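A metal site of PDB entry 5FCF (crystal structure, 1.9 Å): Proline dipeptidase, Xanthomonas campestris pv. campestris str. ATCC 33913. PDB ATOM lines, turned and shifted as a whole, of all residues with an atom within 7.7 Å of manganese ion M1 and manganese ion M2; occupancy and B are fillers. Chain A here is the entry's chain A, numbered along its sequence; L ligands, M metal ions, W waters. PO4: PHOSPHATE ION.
The backbone carbonyl oxygen of Thr 264 is in hydrogen-bond range of the backbone NH of Glu 374. NE2 of His 376 lies close to OE2 of Glu 374 (3.0 Å). O of Asp 262 sits at hydrogen-bond distance from NE2 of His 376 (2.9 Å). The side-chain carboxylate (OD2) of Asp 251 lies close to the side-chain hydroxyl (OG1) of Thr 264 (2.9 Å). The side-chain carboxylate (OD2) of Asp 251 sits close to the guanidinium group (NH2) of Arg 372 (2.8 Å). O of Asp 251 sits at hydrogen-bond distance from N of Ile 223. The backbone carbonyl oxygen (O) of Ile 337 sits close to a ring nitrogen (ND1) of His 331 (3.1 Å). The backbone carbonyl oxygen (O) of Thr 329 sits at hydrogen-bond distance from the backbone NH (N) of Glu 360, at 2.9 Å.
Thr 264 touches manganese ion M2 (OG1 to MN, 3.7 Å). Four residues have an atom within 4 Å of manganese ion M2: Asp 251, Asp 262, Thr 264 and Glu 374.
Manganese ion M2 is bound by O1 of the ligand (1.8 Å), OD1 of Asp 262 (2.1 Å), OD1 of Asp 251 (2.2 Å), OE1 of Glu 374 (2.2 Å), OD2 of Asp 251 (2.3 Å) and water W1 (2.4 Å). Manganese ion M2 has six donor atoms within binding distance.
Manganese ion M1 is bound by the side-chain carboxylate of Glu 374 (2.1 Å), the side-chain carboxylate of Asp 262 (2.1 Å), an oxygen (O1) of the ligand (2.2 Å), a ring nitrogen (NE2) of His 331 (2.2 Å) and the side-chain carboxylate of Glu 360 (2.2 Å).
Residues that only touch manganese ion M1: Ser 358 (3.97 Å). The nearest printed residue that does not touch manganese ion M1 is His 376 (4.1 Å).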
ATOM      1  N   PHE A 221      14.810  20.305 -31.029  1.00  0.00           N
ATOM      2  CA  PHE A 221      14.498  19.804 -32.407  1.00  0.00           C
ATOM      3  C   PHE A 221      12.971  19.954 -32.541  1.00  0.00           C
ATOM      4  O   PHE A 221      12.287  20.092 -31.502  1.00  0.00           O
ATOM      5  CB  PHE A 221      14.871  18.322 -32.592  1.00  0.00           C
ATOM      6  CG  PHE A 221      14.119  17.423 -31.635  1.00  0.00           C
ATOM      7  CD1 PHE A 221      14.677  17.178 -30.367  1.00  0.00           C
ATOM      8  CD2 PHE A 221      12.911  16.819 -31.979  1.00  0.00           C
ATOM      9  CE1 PHE A 221      14.026  16.369 -29.401  1.00  0.00           C
ATOM     10  CE2 PHE A 221      12.225  16.031 -31.018  1.00  0.00           C
ATOM     11  CZ  PHE A 221      12.803  15.840 -29.727  1.00  0.00           C
ATOM     12  N   ILE A 223       9.808  18.136 -35.155  1.00  0.00           N
ATOM     13  CA  ILE A 223       9.259  17.500 -36.379  1.00  0.00           C
ATOM     14  C   ILE A 223       7.779  17.640 -36.356  1.00  0.00           C
ATOM     15  O   ILE A 223       7.146  17.332 -35.306  1.00  0.00           O
ATOM     16  CB  ILE A 223       9.570  16.026 -36.356  1.00  0.00           C
ATOM     17  CG1 ILE A 223      11.102  15.872 -36.387  1.00  0.00           C
ATOM     18  CG2 ILE A 223       8.921  15.319 -37.600  1.00  0.00           C
ATOM     19  CD1 ILE A 223      11.454  14.408 -36.305  1.00  0.00           C
ATOM     20  N   HIS A 234      10.947   9.423 -39.427  1.00  0.00           N
ATOM     21  CA  HIS A 234      11.573  10.734 -39.385  1.00  0.00           C
ATOM     22  C   HIS A 234      11.310  11.726 -40.476  1.00  0.00           C
ATOM     23  O   HIS A 234      11.954  12.685 -40.481  1.00  0.00           O
ATOM     24  CB  HIS A 234      13.017  10.575 -39.111  1.00  0.00           C
ATOM     25  CG  HIS A 234      13.261  10.147 -37.684  1.00  0.00           C
ATOM     26  ND1 HIS A 234      14.166   9.134 -37.343  1.00  0.00           N
ATOM     27  CD2 HIS A 234      12.631  10.524 -36.514  1.00  0.00           C
ATOM     28  CE1 HIS A 234      14.080   8.921 -36.040  1.00  0.00           C
ATOM     29  NE2 HIS A 234      13.210   9.785 -35.508  1.00  0.00           N
ATOM     30  N   ILE A 250       3.577  15.630 -34.010  1.00  0.00           N
ATOM     31  CA  ILE A 250       4.510  16.609 -33.527  1.00  0.00           C
ATOM     32  C   ILE A 250       5.429  15.922 -32.535  1.00  0.00           C
ATOM     33  O   ILE A 250       5.011  15.316 -31.556  1.00  0.00           O
ATOM     34  CB  ILE A 250       3.805  17.710 -32.799  1.00  0.00           C
ATOM     35  CG1 ILE A 250       2.861  18.489 -33.763  1.00  0.00           C
ATOM     36  CG2 ILE A 250       4.793  18.717 -32.261  1.00  0.00           C
ATOM     37  CD1 ILE A 250       2.054  19.594 -33.157  1.00  0.00           C
ATOM     38  N   ASP A 251       6.723  16.004 -32.842  1.00  0.00           N
ATOM     39  CA  ASP A 251       7.759  15.385 -32.002  1.00  0.00           C
ATOM     40  C   ASP A 251       8.747  16.532 -31.693  1.00  0.00           C
ATOM     41  O   ASP A 251       9.311  17.122 -32.643  1.00  0.00           O
ATOM     42  CB  ASP A 251       8.414  14.172 -32.705  1.00  0.00           C
ATOM     43  CG  ASP A 251       9.455  13.460 -31.844  1.00  0.00           C
ATOM     44  OD1 ASP A 251       9.770  13.882 -30.678  1.00  0.00           O
ATOM     45  OD2 ASP A 251       9.890  12.396 -32.228  1.00  0.00           O
ATOM     46  N   THR A 252       8.922  16.895 -30.417  1.00  0.00           N
ATOM     47  CA  THR A 252       9.747  18.048 -30.096  1.00  0.00           C
ATOM     48  C   THR A 252      10.278  17.891 -28.672  1.00  0.00           C
ATOM     49  O   THR A 252       9.873  16.964 -27.892  1.00  0.00           O
ATOM     50  CB  THR A 252       8.960  19.386 -30.249  1.00  0.00           C
ATOM     51  OG1 THR A 252       9.875  20.524 -30.186  1.00  0.00           O
ATOM     52  CG2 THR A 252       7.771  19.504 -29.287  1.00  0.00           C
ATOM     53  N   GLY A 253      11.102  18.828 -28.284  1.00  0.00           N
ATOM     54  CA  GLY A 253      11.735  18.765 -26.980  1.00  0.00           C
ATOM     55  C   GLY A 253      12.638  20.010 -26.764  1.00  0.00           C
ATOM     56  O   GLY A 253      12.864  20.789 -27.707  1.00  0.00           O
ATOM     57  N   SER A 261      13.993  16.774 -22.778  1.00  0.00           N
ATOM     58  CA  SER A 261      12.711  16.208 -23.140  1.00  0.00           C
ATOM     59  C   SER A 261      12.630  15.784 -24.637  1.00  0.00           C
ATOM     60  O   SER A 261      13.487  16.085 -25.491  1.00  0.00           O
ATOM     61  CB  SER A 261      11.599  17.212 -22.792  1.00  0.00           C
ATOM     62  OG  SER A 261      11.691  18.318 -23.622  1.00  0.00           O
ATOM     63  N   ASP A 262      11.626  14.961 -24.911  1.00  0.00           N
ATOM     64  CA  ASP A 262      11.536  14.277 -26.199  1.00  0.00           C
ATOM     65  C   ASP A 262      10.156  13.586 -26.273  1.00  0.00           C
ATOM     66  O   ASP A 262      10.012  12.520 -25.753  1.00  0.00           O
ATOM     67  CB  ASP A 262      12.755  13.288 -26.399  1.00  0.00           C
ATOM     68  CG  ASP A 262      12.633  12.463 -27.630  1.00  0.00           C
ATOM     69  OD1 ASP A 262      11.886  12.939 -28.551  1.00  0.00           O
ATOM     70  OD2 ASP A 262      13.173  11.298 -27.713  1.00  0.00           O
ATOM     71  N   ILE A 263       9.172  14.314 -26.745  1.00  0.00           N
ATOM     72  CA  ILE A 263       7.774  13.883 -26.673  1.00  0.00           C
ATOM     73  C   ILE A 263       7.094  13.974 -28.016  1.00  0.00           C
ATOM     74  O   ILE A 263       7.277  15.004 -28.742  1.00  0.00           O
ATOM     75  CB  ILE A 263       7.014  14.775 -25.698  1.00  0.00           C
ATOM     76  CG1 ILE A 263       7.552  14.704 -24.261  1.00  0.00           C
ATOM     77  CG2 ILE A 263       5.552  14.350 -25.669  1.00  0.00           C
ATOM     78  CD1 ILE A 263       7.059  15.816 -23.327  1.00  0.00           C
ATOM     79  N   THR A 264       6.309  12.903 -28.353  1.00  0.00           N
ATOM     80  CA  THR A 264       5.601  12.914 -29.588  1.00  0.00           C
ATOM     81  C   THR A 264       4.153  12.813 -29.237  1.00  0.00           C
ATOM     82  O   THR A 264       3.787  11.969 -28.372  1.00  0.00           O
ATOM     83  CB  THR A 264       5.982  11.785 -30.577  1.00  0.00           C
ATOM     84  OG1 THR A 264       7.408  11.779 -30.795  1.00  0.00           O
ATOM     85  CG2 THR A 264       5.258  11.990 -31.883  1.00  0.00           C
ATOM     86  N   ARG A 328      12.917   0.179 -33.118  1.00  0.00           N
ATOM     87  CA  ARG A 328      12.899  -0.249 -31.710  1.00  0.00           C
ATOM     88  C   ARG A 328      11.785   0.508 -30.935  1.00  0.00           C
ATOM     89  O   ARG A 328      11.227   1.607 -31.363  1.00  0.00           O
ATOM     90  CB  ARG A 328      14.277   0.092 -31.153  1.00  0.00           C
ATOM     91  CG  ARG A 328      14.476   1.614 -30.901  1.00  0.00           C
ATOM     92  CD  ARG A 328      15.926   2.069 -30.661  1.00  0.00           C
ATOM     93  NE  ARG A 328      15.934   3.531 -30.651  1.00  0.00           N
ATOM     94  CZ  ARG A 328      16.996   4.264 -30.955  1.00  0.00           C
ATOM     95  NH1 ARG A 328      18.153   3.698 -31.199  1.00  0.00           N
ATOM     96  NH2 ARG A 328      16.852   5.564 -31.101  1.00  0.00           N
ATOM     97  N   THR A 329      11.418  -0.058 -29.791  1.00  0.00           N
ATOM     98  CA  THR A 329      10.397   0.565 -28.956  1.00  0.00           C
ATOM     99  C   THR A 329      10.799   1.897 -28.257  1.00  0.00           C
ATOM    100  O   THR A 329       9.981   2.821 -28.066  1.00  0.00           O
ATOM    101  CB  THR A 329       9.912  -0.474 -27.944  1.00  0.00           C
ATOM    102  OG1 THR A 329       9.095  -1.407 -28.667  1.00  0.00           O
ATOM    103  CG2 THR A 329       9.032   0.047 -26.828  1.00  0.00           C
ATOM    104  N   GLY A 330      12.090   2.051 -27.930  1.00  0.00           N
ATOM    105  CA  GLY A 330      12.536   3.213 -27.214  1.00  0.00           C
ATOM    106  C   GLY A 330      14.053   3.246 -27.009  1.00  0.00           C
ATOM    107  O   GLY A 330      14.784   2.253 -27.355  1.00  0.00           O
ATOM    108  N   HIS A 331      14.490   4.390 -26.482  1.00  0.00           N
ATOM    109  CA  HIS A 331      15.839   4.689 -26.239  1.00  0.00           C
ATOM    110  C   HIS A 331      16.018   5.318 -24.908  1.00  0.00           C
ATOM    111  O   HIS A 331      15.223   6.080 -24.477  1.00  0.00           O
ATOM    112  CB  HIS A 331      16.457   5.540 -27.349  1.00  0.00           C
ATOM    113  CG  HIS A 331      15.762   6.851 -27.525  1.00  0.00           C
ATOM    114  ND1 HIS A 331      15.981   7.948 -26.737  1.00  0.00           N
ATOM    115  CD2 HIS A 331      14.701   7.151 -28.329  1.00  0.00           C
ATOM    116  CE1 HIS A 331      15.150   8.911 -27.092  1.00  0.00           C
ATOM    117  NE2 HIS A 331      14.348   8.471 -28.054  1.00  0.00           N
ATOM    118  N   GLY A 332      17.190   5.156 -24.368  1.00  0.00           N
ATOM    119  CA  GLY A 332      17.626   6.018 -23.268  1.00  0.00           C
ATOM    120  C   GLY A 332      17.693   7.484 -23.571  1.00  0.00           C
ATOM    121  O   GLY A 332      17.863   7.934 -24.708  1.00  0.00           O
ATOM    122  N   CYS A 333      17.502   8.281 -22.494  1.00  0.00           N
ATOM    123  CA  CYS A 333      17.518   9.737 -22.599  1.00  0.00           C
ATOM    124  C   CYS A 333      18.173  10.312 -21.375  1.00  0.00           C
ATOM    125  O   CYS A 333      18.054   9.766 -20.252  1.00  0.00           O
ATOM    126  CB  CYS A 333      16.102  10.251 -22.790  1.00  0.00           C
ATOM    127  SG  CYS A 333      15.981  11.973 -23.293  1.00  0.00           S
ATOM    128  N   ILE A 337      19.794  13.186 -26.320  1.00  0.00           N
ATOM    129  CA  ILE A 337      18.506  12.712 -26.703  1.00  0.00           C
ATOM    130  C   ILE A 337      18.448  11.176 -26.747  1.00  0.00           C
ATOM    131  O   ILE A 337      17.461  10.584 -26.219  1.00  0.00           O
ATOM    132  CB  ILE A 337      18.030  13.263 -28.094  1.00  0.00           C
ATOM    133  CG1 ILE A 337      17.992  14.780 -28.076  1.00  0.00           C
ATOM    134  CG2 ILE A 337      16.610  12.725 -28.382  1.00  0.00           C
ATOM    135  CD1 ILE A 337      17.832  15.501 -29.392  1.00  0.00           C
ATOM    136  N   HIS A 338      19.418  10.578 -27.414  1.00  0.00           N
ATOM    137  CA  HIS A 338      19.520   9.153 -27.531  1.00  0.00           C
ATOM    138  C   HIS A 338      20.776   8.727 -26.729  1.00  0.00           C
ATOM    139  O   HIS A 338      21.854   9.183 -27.068  1.00  0.00           O
ATOM    140  CB  HIS A 338      19.651   8.759 -28.985  1.00  0.00           C
ATOM    141  CG  HIS A 338      18.509   9.228 -29.785  1.00  0.00           C
ATOM    142  ND1 HIS A 338      18.572  10.387 -30.565  1.00  0.00           N
ATOM    143  CD2 HIS A 338      17.199   8.864 -29.772  1.00  0.00           C
ATOM    144  CE1 HIS A 338      17.359  10.594 -31.107  1.00  0.00           C
ATOM    145  NE2 HIS A 338      16.554   9.597 -30.738  1.00  0.00           N
ATOM    146  N   ALA A 357      14.033   6.093 -20.190  1.00  0.00           N
ATOM    147  CA  ALA A 357      13.935   5.765 -21.616  1.00  0.00           C
ATOM    148  C   ALA A 357      12.618   6.213 -22.194  1.00  0.00           C
ATOM    149  O   ALA A 357      11.657   6.459 -21.415  1.00  0.00           O
ATOM    150  CB  ALA A 357      14.081   4.259 -21.801  1.00  0.00           C
ATOM    151  N   SER A 358      12.621   6.404 -23.502  1.00  0.00           N
ATOM    152  CA  SER A 358      11.410   6.615 -24.301  1.00  0.00           C
ATOM    153  C   SER A 358      10.590   5.373 -24.500  1.00  0.00           C
ATOM    154  O   SER A 358      11.072   4.209 -24.412  1.00  0.00           O
ATOM    155  CB  SER A 358      11.732   7.219 -25.669  1.00  0.00           C
ATOM    156  OG  SER A 358      12.244   6.248 -26.539  1.00  0.00           O
ATOM    157  N   ASN A 359       9.298   5.596 -24.690  1.00  0.00           N
ATOM    158  CA  ASN A 359       8.374   4.487 -24.942  1.00  0.00           C
ATOM    159  C   ASN A 359       7.484   4.996 -26.118  1.00  0.00           C
ATOM    160  O   ASN A 359       6.574   5.844 -25.962  1.00  0.00           O
ATOM    161  CB  ASN A 359       7.544   4.184 -23.709  1.00  0.00           C
ATOM    162  CG  ASN A 359       6.607   2.973 -23.898  1.00  0.00           C
ATOM    163  OD1 ASN A 359       6.407   2.513 -25.031  1.00  0.00           O
ATOM    164  ND2 ASN A 359       5.933   2.565 -22.821  1.00  0.00           N
ATOM    165  N   GLU A 360       7.826   4.559 -27.324  1.00  0.00           N
ATOM    166  CA  GLU A 360       7.416   5.236 -28.580  1.00  0.00           C
ATOM    167  C   GLU A 360       7.295   4.161 -29.713  1.00  0.00           C
ATOM    168  O   GLU A 360       7.903   4.247 -30.755  1.00  0.00           O
ATOM    169  CB  GLU A 360       8.320   6.400 -28.942  1.00  0.00           C
ATOM    170  CG  GLU A 360       9.799   6.090 -28.884  1.00  0.00           C
ATOM    171  CD  GLU A 360      10.645   7.182 -29.466  1.00  0.00           C
ATOM    172  OE1 GLU A 360      10.250   7.695 -30.539  1.00  0.00           O
ATOM    173  OE2 GLU A 360      11.691   7.515 -28.923  1.00  0.00           O
ATOM    174  N   ARG A 372       2.650   7.833 -33.822  1.00  0.00           N
ATOM    175  CA  ARG A 372       3.698   7.652 -32.836  1.00  0.00           C
ATOM    176  C   ARG A 372       3.201   8.369 -31.583  1.00  0.00           C
ATOM    177  O   ARG A 372       2.918   9.567 -31.647  1.00  0.00           O
ATOM    178  CB  ARG A 372       5.086   8.197 -33.256  1.00  0.00           C
ATOM    179  CG  ARG A 372       6.139   7.986 -32.117  1.00  0.00           C
ATOM    180  CD  ARG A 372       7.560   8.209 -32.557  1.00  0.00           C
ATOM    181  NE  ARG A 372       7.899   9.579 -32.984  1.00  0.00           N
ATOM    182  CZ  ARG A 372       8.146  10.013 -34.244  1.00  0.00           C
ATOM    183  NH1 ARG A 372       7.811   9.252 -35.290  1.00  0.00           N
ATOM    184  NH2 ARG A 372       8.661  11.255 -34.458  1.00  0.00           N
ATOM    185  N   GLU A 374       4.765   9.106 -27.963  1.00  0.00           N
ATOM    186  CA  GLU A 374       6.056   9.128 -27.235  1.00  0.00           C
ATOM    187  C   GLU A 374       5.991   9.875 -25.933  1.00  0.00           C
ATOM    188  O   GLU A 374       5.816  11.097 -25.906  1.00  0.00           O
ATOM    189  CB  GLU A 374       7.216   9.692 -28.121  1.00  0.00           C
ATOM    190  CG  GLU A 374       8.537   9.744 -27.337  1.00  0.00           C
ATOM    191  CD  GLU A 374       9.744  10.291 -28.139  1.00  0.00           C
ATOM    192  OE1 GLU A 374       9.463  11.070 -29.091  1.00  0.00           O
ATOM    193  OE2 GLU A 374      10.863   9.920 -27.696  1.00  0.00           O
ATOM    194  N   ASP A 375       6.187   9.119 -24.858  1.00  0.00           N
ATOM    195  CA  ASP A 375       6.373   9.627 -23.503  1.00  0.00           C
ATOM    196  C   ASP A 375       7.563   8.817 -22.911  1.00  0.00           C
ATOM    197  O   ASP A 375       7.822   7.634 -23.310  1.00  0.00           O
ATOM    198  CB  ASP A 375       5.119   9.418 -22.707  1.00  0.00           C
ATOM    199  CG  ASP A 375       3.891  10.106 -23.325  1.00  0.00           C
ATOM    200  OD1 ASP A 375       3.253   9.607 -24.358  1.00  0.00           O
ATOM    201  OD2 ASP A 375       3.642  11.206 -22.810  1.00  0.00           O
ATOM    202  N   HIS A 376       8.318   9.480 -22.044  1.00  0.00           N
ATOM    203  CA  HIS A 376       9.438   8.826 -21.372  1.00  0.00           C
ATOM    204  C   HIS A 376       9.037   8.423 -19.968  1.00  0.00           C
ATOM    205  O   HIS A 376       8.096   9.019 -19.378  1.00  0.00           O
ATOM    206  CB  HIS A 376      10.607   9.801 -21.322  1.00  0.00           C
ATOM    207  CG  HIS A 376      11.208  10.047 -22.676  1.00  0.00           C
ATOM    208  ND1 HIS A 376      12.566  10.224 -22.867  1.00  0.00           N
ATOM    209  CD2 HIS A 376      10.643  10.104 -23.901  1.00  0.00           C
ATOM    210  CE1 HIS A 376      12.815  10.424 -24.126  1.00  0.00           C
ATOM    211  NE2 HIS A 376      11.672  10.351 -24.796  1.00  0.00           N
HETATM  212  P   PO4 L   1      12.786   9.718 -31.691  1.00  0.00           P
HETATM  213  O1  PO4 L   1      12.041  10.654 -30.559  1.00  0.00           O
HETATM  214  O2  PO4 L   1      13.039  10.608 -32.873  1.00  0.00           O
HETATM  215  O3  PO4 L   1      14.038   8.879 -31.510  1.00  0.00           O
HETATM  216  O4  PO4 L   1      11.769   8.706 -32.223  1.00  0.00           O
HETATM  217 MN    MN M   1      12.578   9.555 -28.765  1.00  0.00          MN
HETATM  218 MN    MN M   2      11.013  12.149 -30.284  1.00  0.00          MN
HETATM  219  O   HOH W   1      12.808  12.939 -31.697  1.00  0.00           O
